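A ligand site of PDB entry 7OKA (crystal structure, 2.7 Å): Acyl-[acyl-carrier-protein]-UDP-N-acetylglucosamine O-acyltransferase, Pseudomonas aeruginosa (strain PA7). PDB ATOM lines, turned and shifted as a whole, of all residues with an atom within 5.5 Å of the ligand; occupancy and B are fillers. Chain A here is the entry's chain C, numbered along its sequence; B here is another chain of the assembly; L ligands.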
ATOM      1  N   LEU A 115      12.304  21.816 -14.561  1.00  0.00           N
ATOM      2  CA  LEU A 115      11.743  21.250 -13.340  1.00  0.00           C
ATOM      3  C   LEU A 115      10.472  20.497 -13.769  1.00  0.00           C
ATOM      4  O   LEU A 115       9.536  21.125 -14.290  1.00  0.00           O
ATOM      5  CB  LEU A 115      11.491  22.410 -12.394  1.00  0.00           C
ATOM      6  CG  LEU A 115      10.774  22.039 -11.108  1.00  0.00           C
ATOM      7  CD1 LEU A 115      11.488  20.886 -10.443  1.00  0.00           C
ATOM      8  CD2 LEU A 115      10.678  23.225 -10.181  1.00  0.00           C
ATOM      9  N   MET A 117       7.680  18.169 -12.341  1.00  0.00           N
ATOM     10  CA  MET A 117       7.117  17.823 -11.039  1.00  0.00           C
ATOM     11  C   MET A 117       6.363  16.505 -11.115  1.00  0.00           C
ATOM     12  O   MET A 117       6.282  15.884 -12.160  1.00  0.00           O
ATOM     13  CB  MET A 117       6.212  18.964 -10.604  1.00  0.00           C
ATOM     14  CG  MET A 117       6.991  20.238 -10.321  1.00  0.00           C
ATOM     15  SD  MET A 117       5.898  21.326  -9.450  1.00  0.00           S
ATOM     16  CE  MET A 117       6.941  22.748  -9.211  1.00  0.00           C
ATOM     17  N   ILE A 133       9.055  24.695 -16.542  1.00  0.00           N
ATOM     18  CA  ILE A 133       8.458  24.044 -15.358  1.00  0.00           C
ATOM     19  C   ILE A 133       7.176  23.345 -15.816  1.00  0.00           C
ATOM     20  O   ILE A 133       6.256  24.034 -16.172  1.00  0.00           O
ATOM     21  CB  ILE A 133       8.166  25.078 -14.264  1.00  0.00           C
ATOM     22  CG1 ILE A 133       9.405  25.897 -13.957  1.00  0.00           C
ATOM     23  CG2 ILE A 133       7.627  24.409 -13.007  1.00  0.00           C
ATOM     24  CD1 ILE A 133       9.223  26.827 -12.794  1.00  0.00           C
ATOM     25  N   VAL A 135       4.466  21.411 -13.998  1.00  0.00           N
ATOM     26  CA  VAL A 135       3.942  21.183 -12.632  1.00  0.00           C
ATOM     27  C   VAL A 135       3.247  19.824 -12.671  1.00  0.00           C
ATOM     28  O   VAL A 135       3.069  19.278 -13.758  1.00  0.00           O
ATOM     29  CB  VAL A 135       3.023  22.323 -12.193  1.00  0.00           C
ATOM     30  CG1 VAL A 135       2.426  22.107 -10.837  1.00  0.00           C
ATOM     31  CG2 VAL A 135       3.768  23.641 -12.183  1.00  0.00           C
ATOM     32  N   ASN A 136       2.988  19.279 -11.488  1.00  0.00           N
ATOM     33  CA  ASN A 136       2.420  17.940 -11.239  1.00  0.00           C
ATOM     34  C   ASN A 136       1.449  17.526 -12.336  1.00  0.00           C
ATOM     35  O   ASN A 136       0.532  18.291 -12.670  1.00  0.00           O
ATOM     36  CB  ASN A 136       1.650  17.947  -9.940  1.00  0.00           C
ATOM     37  CG  ASN A 136       2.495  18.137  -8.704  1.00  0.00           C
ATOM     38  OD1 ASN A 136       3.488  18.854  -8.696  1.00  0.00           O
ATOM     39  ND2 ASN A 136       2.017  17.578  -7.611  1.00  0.00           N
ATOM     40  N   ILE A 151       5.770  27.499 -18.532  1.00  0.00           N
ATOM     41  CA  ILE A 151       5.269  26.996 -17.260  1.00  0.00           C
ATOM     42  C   ILE A 151       3.950  26.367 -17.573  1.00  0.00           C
ATOM     43  O   ILE A 151       3.132  27.054 -18.117  1.00  0.00           O
ATOM     44  CB  ILE A 151       5.156  28.183 -16.337  1.00  0.00           C
ATOM     45  CG1 ILE A 151       6.545  28.783 -16.210  1.00  0.00           C
ATOM     46  CG2 ILE A 151       4.508  27.777 -15.026  1.00  0.00           C
ATOM     47  CD1 ILE A 151       6.661  29.693 -15.031  1.00  0.00           C
ATOM     48  N   LEU A 152       3.845  25.062 -17.436  1.00  0.00           N
ATOM     49  CA  LEU A 152       2.564  24.357 -17.588  1.00  0.00           C
ATOM     50  C   LEU A 152       2.109  24.104 -16.168  1.00  0.00           C
ATOM     51  O   LEU A 152       2.892  23.401 -15.426  1.00  0.00           O
ATOM     52  CB  LEU A 152       2.805  23.087 -18.403  1.00  0.00           C
ATOM     53  CG  LEU A 152       3.365  23.287 -19.810  1.00  0.00           C
ATOM     54  CD1 LEU A 152       2.957  22.140 -20.727  1.00  0.00           C
ATOM     55  CD2 LEU A 152       2.821  24.542 -20.439  1.00  0.00           C
ATOM     56  N   SER A 153       1.013  24.748 -15.745  1.00  0.00           N
ATOM     57  CA  SER A 153       0.448  24.596 -14.373  1.00  0.00           C
ATOM     58  C   SER A 153       0.036  23.126 -14.158  1.00  0.00           C
ATOM     59  O   SER A 153      -0.088  22.362 -15.135  1.00  0.00           O
ATOM     60  CB  SER A 153      -0.679  25.568 -14.161  1.00  0.00           C
ATOM     61  OG  SER A 153      -0.233  26.885 -13.809  1.00  0.00           O
ATOM     62  N   GLY A 154      -0.178  22.719 -12.905  1.00  0.00           N
ATOM     63  CA  GLY A 154      -0.716  21.384 -12.548  1.00  0.00           C
ATOM     64  C   GLY A 154      -1.755  20.845 -13.533  1.00  0.00           C
ATOM     65  O   GLY A 154      -2.683  21.612 -13.920  1.00  0.00           O
ATOM     66  N   TYR A 155      -1.619  19.557 -13.920  1.00  0.00           N
ATOM     67  CA  TYR A 155      -2.635  18.790 -14.691  1.00  0.00           C
ATOM     68  C   TYR A 155      -2.949  19.466 -16.040  1.00  0.00           C
ATOM     69  O   TYR A 155      -4.088  19.326 -16.567  1.00  0.00           O
ATOM     70  CB  TYR A 155      -3.929  18.652 -13.901  1.00  0.00           C
ATOM     71  CG  TYR A 155      -3.794  17.665 -12.789  1.00  0.00           C
ATOM     72  CD1 TYR A 155      -3.116  17.979 -11.600  1.00  0.00           C
ATOM     73  CD2 TYR A 155      -4.307  16.411 -12.927  1.00  0.00           C
ATOM     74  CE1 TYR A 155      -2.962  17.050 -10.576  1.00  0.00           C
ATOM     75  CE2 TYR A 155      -4.143  15.475 -11.922  1.00  0.00           C
ATOM     76  CZ  TYR A 155      -3.468  15.780 -10.749  1.00  0.00           C
ATOM     77  OH  TYR A 155      -3.375  14.807  -9.814  1.00  0.00           O
ATOM     78  N   PHE A 169       2.342  30.186 -20.623  1.00  0.00           N
ATOM     79  CA  PHE A 169       1.911  29.761 -19.285  1.00  0.00           C
ATOM     80  C   PHE A 169       0.523  29.196 -19.370  1.00  0.00           C
ATOM     81  O   PHE A 169      -0.308  29.890 -19.882  1.00  0.00           O
ATOM     82  CB  PHE A 169       1.885  30.952 -18.350  1.00  0.00           C
ATOM     83  CG  PHE A 169       1.302  30.647 -17.019  1.00  0.00           C
ATOM     84  CD1 PHE A 169      -0.070  30.599 -16.842  1.00  0.00           C
ATOM     85  CD2 PHE A 169       2.115  30.415 -15.935  1.00  0.00           C
ATOM     86  CE1 PHE A 169      -0.605  30.274 -15.600  1.00  0.00           C
ATOM     87  CE2 PHE A 169       1.569  30.112 -14.690  1.00  0.00           C
ATOM     88  CZ  PHE A 169       0.211  30.041 -14.530  1.00  0.00           C
ATOM     89  N   MET A 172      -4.061  25.830 -14.217  1.00  0.00           N
ATOM     90  CA  MET A 172      -4.223  24.441 -13.810  1.00  0.00           C
ATOM     91  C   MET A 172      -5.379  23.835 -14.575  1.00  0.00           C
ATOM     92  O   MET A 172      -6.389  24.465 -14.742  1.00  0.00           O
ATOM     93  CB  MET A 172      -4.354  24.243 -12.303  1.00  0.00           C
ATOM     94  CG  MET A 172      -5.396  25.054 -11.621  1.00  0.00           C
ATOM     95  SD  MET A 172      -5.457  24.316  -9.985  1.00  0.00           S
ATOM     96  CE  MET A 172      -7.082  25.001  -9.623  1.00  0.00           C
ATOM     97  N   PRO B  72       9.130  20.983  -4.530  1.00  0.00           N
ATOM     98  CA  PRO B  72      10.048  21.432  -5.568  1.00  0.00           C
ATOM     99  C   PRO B  72       9.952  22.928  -5.860  1.00  0.00           C
ATOM    100  O   PRO B  72      10.771  23.328  -6.617  1.00  0.00           O
ATOM    101  CB  PRO B  72       9.609  20.623  -6.798  1.00  0.00           C
ATOM    102  CG  PRO B  72       8.155  20.537  -6.592  1.00  0.00           C
ATOM    103  CD  PRO B  72       8.070  20.196  -5.113  1.00  0.00           C
ATOM    104  N   ASP B  73       8.962  23.636  -5.274  1.00  0.00           N
ATOM    105  CA  ASP B  73       8.664  25.066  -5.546  1.00  0.00           C
ATOM    106  C   ASP B  73       9.969  25.848  -5.309  1.00  0.00           C
ATOM    107  O   ASP B  73      10.592  25.702  -4.244  1.00  0.00           O
ATOM    108  CB  ASP B  73       7.514  25.607  -4.697  1.00  0.00           C
ATOM    109  CG  ASP B  73       6.056  25.518  -5.203  1.00  0.00           C
ATOM    110  OD1 ASP B  73       5.309  26.565  -4.929  1.00  0.00           O
ATOM    111  OD2 ASP B  73       5.610  24.394  -5.761  1.00  0.00           O
ATOM    112  N   LEU B  74      10.364  26.666  -6.290  1.00  0.00           N
ATOM    113  CA  LEU B  74      11.674  27.377  -6.314  1.00  0.00           C
ATOM    114  C   LEU B  74      11.794  28.305  -5.092  1.00  0.00           C
ATOM    115  O   LEU B  74      12.928  28.584  -4.724  1.00  0.00           O
ATOM    116  CB  LEU B  74      11.775  28.129  -7.652  1.00  0.00           C
ATOM    117  CG  LEU B  74      12.497  27.476  -8.846  1.00  0.00           C
ATOM    118  CD1 LEU B  74      12.463  25.964  -8.850  1.00  0.00           C
ATOM    119  CD2 LEU B  74      11.906  27.988 -10.153  1.00  0.00           C
ATOM    120  N   LYS B  75      10.654  28.693  -4.510  1.00  0.00           N
ATOM    121  CA  LYS B  75      10.518  29.625  -3.366  1.00  0.00           C
ATOM    122  C   LYS B  75      11.179  28.992  -2.134  1.00  0.00           C
ATOM    123  O   LYS B  75      11.828  29.709  -1.395  1.00  0.00           O
ATOM    124  CB  LYS B  75       9.030  29.943  -3.167  1.00  0.00           C
ATOM    125  CG  LYS B  75       8.475  30.002  -1.746  1.00  0.00           C
ATOM    126  CD  LYS B  75       7.160  29.204  -1.475  1.00  0.00           C
ATOM    127  CE  LYS B  75       5.877  29.756  -2.073  1.00  0.00           C
ATOM    128  NZ  LYS B  75       4.928  30.209  -1.020  1.00  0.00           N
ATOM    129  N   HIS B 121      -2.262  14.672  -3.987  1.00  0.00           N
ATOM    130  CA  HIS B 121      -1.059  15.482  -3.680  1.00  0.00           C
ATOM    131  C   HIS B 121      -1.432  16.572  -2.703  1.00  0.00           C
ATOM    132  O   HIS B 121      -2.402  17.325  -2.996  1.00  0.00           O
ATOM    133  CB  HIS B 121      -0.469  16.093  -4.928  1.00  0.00           C
ATOM    134  CG  HIS B 121       0.447  17.207  -4.638  1.00  0.00           C
ATOM    135  ND1 HIS B 121       1.763  17.000  -4.317  1.00  0.00           N
ATOM    136  CD2 HIS B 121       0.241  18.539  -4.604  1.00  0.00           C
ATOM    137  CE1 HIS B 121       2.358  18.168  -4.160  1.00  0.00           C
ATOM    138  NE2 HIS B 121       1.444  19.141  -4.337  1.00  0.00           N
ATOM    139  N   ALA B 139      -5.505  17.376  -5.864  1.00  0.00           N
ATOM    140  CA  ALA B 139      -4.222  18.098  -5.765  1.00  0.00           C
ATOM    141  C   ALA B 139      -4.374  19.446  -5.045  1.00  0.00           C
ATOM    142  O   ALA B 139      -5.006  20.357  -5.598  1.00  0.00           O
ATOM    143  CB  ALA B 139      -3.731  18.288  -7.134  1.00  0.00           C
ATOM    144  N   LEU B 140      -3.838  19.576  -3.836  1.00  0.00           N
ATOM    145  CA  LEU B 140      -3.846  20.881  -3.140  1.00  0.00           C
ATOM    146  C   LEU B 140      -2.555  21.602  -3.496  1.00  0.00           C
ATOM    147  O   LEU B 140      -1.504  21.124  -3.071  1.00  0.00           O
ATOM    148  CB  LEU B 140      -3.972  20.640  -1.642  1.00  0.00           C
ATOM    149  CG  LEU B 140      -5.053  19.638  -1.237  1.00  0.00           C
ATOM    150  CD1 LEU B 140      -5.242  19.664   0.260  1.00  0.00           C
ATOM    151  CD2 LEU B 140      -6.387  19.923  -1.917  1.00  0.00           C
ATOM    152  N   ALA B 141      -2.596  22.686  -4.269  1.00  0.00           N
ATOM    153  CA  ALA B 141      -1.327  23.236  -4.840  1.00  0.00           C
ATOM    154  C   ALA B 141      -0.378  23.706  -3.730  1.00  0.00           C
ATOM    155  O   ALA B 141       0.857  23.558  -3.941  1.00  0.00           O
ATOM    156  CB  ALA B 141      -1.537  24.327  -5.811  1.00  0.00           C
ATOM    157  N   LEU B 157      -8.647  19.871  -8.384  1.00  0.00           N
ATOM    158  CA  LEU B 157      -7.463  20.755  -8.248  1.00  0.00           C
ATOM    159  C   LEU B 157      -7.846  21.988  -7.424  1.00  0.00           C
ATOM    160  O   LEU B 157      -8.898  22.558  -7.697  1.00  0.00           O
ATOM    161  CB  LEU B 157      -7.004  21.199  -9.625  1.00  0.00           C
ATOM    162  CG  LEU B 157      -6.941  20.078 -10.638  1.00  0.00           C
ATOM    163  CD1 LEU B 157      -6.483  20.627 -11.989  1.00  0.00           C
ATOM    164  CD2 LEU B 157      -6.042  18.974 -10.090  1.00  0.00           C
ATOM    165  N   VAL B 158      -7.027  22.331  -6.425  1.00  0.00           N
ATOM    166  CA  VAL B 158      -7.227  23.506  -5.541  1.00  0.00           C
ATOM    167  C   VAL B 158      -6.016  24.414  -5.619  1.00  0.00           C
ATOM    168  O   VAL B 158      -4.916  23.972  -5.318  1.00  0.00           O
ATOM    169  CB  VAL B 158      -7.498  23.064  -4.101  1.00  0.00           C
ATOM    170  CG1 VAL B 158      -7.813  24.259  -3.230  1.00  0.00           C
ATOM    171  CG2 VAL B 158      -8.627  22.046  -4.040  1.00  0.00           C
ATOM    172  N   HIS B 159      -6.276  25.658  -5.961  1.00  0.00           N
ATOM    173  CA  HIS B 159      -5.272  26.722  -6.185  1.00  0.00           C
ATOM    174  C   HIS B 159      -4.685  27.110  -4.827  1.00  0.00           C
ATOM    175  O   HIS B 159      -5.370  26.965  -3.815  1.00  0.00           O
ATOM    176  CB  HIS B 159      -5.945  27.840  -6.990  1.00  0.00           C
ATOM    177  CG  HIS B 159      -5.135  29.071  -7.205  1.00  0.00           C
ATOM    178  ND1 HIS B 159      -5.108  30.136  -6.270  1.00  0.00           N
ATOM    179  CD2 HIS B 159      -4.382  29.453  -8.252  1.00  0.00           C
ATOM    180  CE1 HIS B 159      -4.362  31.128  -6.725  1.00  0.00           C
ATOM    181  NE2 HIS B 159      -3.913  30.743  -7.959  1.00  0.00           N
ATOM    182  N   GLN B 160      -3.450  27.580  -4.839  1.00  0.00           N
ATOM    183  CA  GLN B 160      -2.755  28.062  -3.625  1.00  0.00           C
ATOM    184  C   GLN B 160      -3.702  28.976  -2.816  1.00  0.00           C
ATOM    185  O   GLN B 160      -4.457  29.759  -3.414  1.00  0.00           O
ATOM    186  CB  GLN B 160      -1.344  28.612  -3.984  1.00  0.00           C
ATOM    187  CG  GLN B 160      -1.214  29.675  -5.103  1.00  0.00           C
ATOM    188  CD  GLN B 160      -1.354  29.281  -6.573  1.00  0.00           C
ATOM    189  OE1 GLN B 160      -1.707  28.158  -7.016  1.00  0.00           O
ATOM    190  NE2 GLN B 160      -1.105  30.291  -7.400  1.00  0.00           N
HETATM  191  C1  LIG L   1       7.260  26.524  -9.214  1.00  0.00           C
HETATM  192  C2  LIG L   1       1.297  22.211  -7.554  1.00  0.00           C
HETATM  193  C3  LIG L   1       0.841  20.914  -7.488  1.00  0.00           C
HETATM  194  C4  LIG L   1       5.716  27.593 -10.714  1.00  0.00           C
HETATM  195  C5  LIG L   1       4.914  25.929  -9.187  1.00  0.00           C
HETATM  196  C6  LIG L   1       4.440  27.755 -11.203  1.00  0.00           C
HETATM  197  C7  LIG L   1       3.628  26.098  -9.657  1.00  0.00           C
HETATM  198  C8  LIG L   1       0.571  23.199  -8.185  1.00  0.00           C
HETATM  199  C9  LIG L   1      -0.371  20.603  -8.052  1.00  0.00           C
HETATM  200  C10 LIG L   1      -1.070  29.093 -11.100  1.00  0.00           C
HETATM  201  C11 LIG L   1      -0.890  31.243 -10.641  1.00  0.00           C
HETATM  202  C12 LIG L   1       5.943  26.683  -9.712  1.00  0.00           C
HETATM  203  C13 LIG L   1       3.394  27.017 -10.676  1.00  0.00           C
HETATM  204  C14 LIG L   1      -0.635  22.898  -8.771  1.00  0.00           C
HETATM  205  C15 LIG L   1      -1.081  21.588  -8.679  1.00  0.00           C
HETATM  206  C16 LIG L   1      -0.079  29.293 -10.161  1.00  0.00           C
HETATM  207  C17 LIG L   1       0.328  25.907 -10.273  1.00  0.00           C
HETATM  208  C18 LIG L   1       2.048  27.245 -11.222  1.00  0.00           C
HETATM  209  C19 LIG L   1       0.806  28.305  -9.444  1.00  0.00           C
HETATM  210  C20 LIG L   1      -0.777  25.668  -9.316  1.00  0.00           C
HETATM  211  N1  LIG L   1       8.304  26.433  -8.746  1.00  0.00           N
HETATM  212  N2  LIG L   1       0.032  30.644  -9.886  1.00  0.00           N
HETATM  213  N3  LIG L   1      -1.582  30.340 -11.403  1.00  0.00           N
HETATM  214  N4  LIG L   1       1.091  27.081 -10.174  1.00  0.00           N
HETATM  215  O1  LIG L   1       0.563  25.044 -11.119  1.00  0.00           O
HETATM  216  S1  LIG L   1      -1.634  24.080  -9.631  1.00  0.00           S
HETATM  217 CL1  LIG L   1      -2.584  21.169  -9.348  1.00  0.00          CL
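Met 117 touches the ligand (CE to C5, 3.8 Å).
CG1 of Val 135 touches C8 of the ligand, at 3.4 Å.
Asn 136 touches the ligand.
Ile 151 touches the ligand.
Tyr 155 touches the ligand (CD1 to CL1, 3.9 Å).
CZ of Phe 169 touches N3 of the ligand (3.6 Å).
Met 172 touches the ligand (CB to S1, 3.8 Å).
Asp 73 of chain B touches the ligand (CA to N1, 3.5 Å).
His 121 of chain B touches the ligand.
Ala 139 of chain B touches the ligand.
Ala 141 of chain B touches the ligand.
Hydrophobic or aromatic side chains within 4 Å of the ligand: Met 117, Val 135, Ile 151, Tyr 155, Phe 169, Met 172, His 121 of chain B, Ala 139 of chain B and Ala 141 of chain B.
The nearest printed residue that does not touch the ligand is His 159 of chain B (4.1 Å).
The backbone NH of Gly 154 sits at hydrogen-bond distance from an oxygen (O1) of the ligand (3.0 Å).
N1 of the ligand sits at hydrogen-bond distance from N of Leu 74 of chain B (3.2 Å).
NE2 of Gln 160 of chain B is in hydrogen-bond range of N2 of the ligand, at 2.8 Å.
OG of Ser 153 lies close to O1 of the ligand.
The backbone carbonyl oxygen of Leu 152 is in hydrogen-bond range of the backbone NH of Val 135 (2.9 Å).
The backbone NH (N) of Ala 141 of chain B sits at hydrogen-bond distance from the backbone carbonyl oxygen (O) of Val 158 of chain B (2.9 Å).
The backbone NH (N) of Leu 140 of chain B sits at hydrogen-bond distance from the backbone carbonyl oxygen (O) of His 121 of chain B, at 2.8 Å.
O of Ala 139 of chain B is in hydrogen-bond range of N of Val 158 of chain B, 2.9 Å away.
The side-chain amide nitrogen of Gln 160 of chain B is in hydrogen-bond range of a ring nitrogen (NE2) of His 159 of chain B, at 2.9 Å.
The side-chain amide oxygen of Asn 136 sits close to the side-chain sulfur of Met 117 (3.5 Å).
The backbone carbonyl oxygen (O) of Asn 136 lies within hydrogen-bond range of the backbone NH (N) of Tyr 155 (2.8 Å).
ND2 of Asn 136 sits at hydrogen-bond distance from ND1 of His 121 of chain B (3.4 Å).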
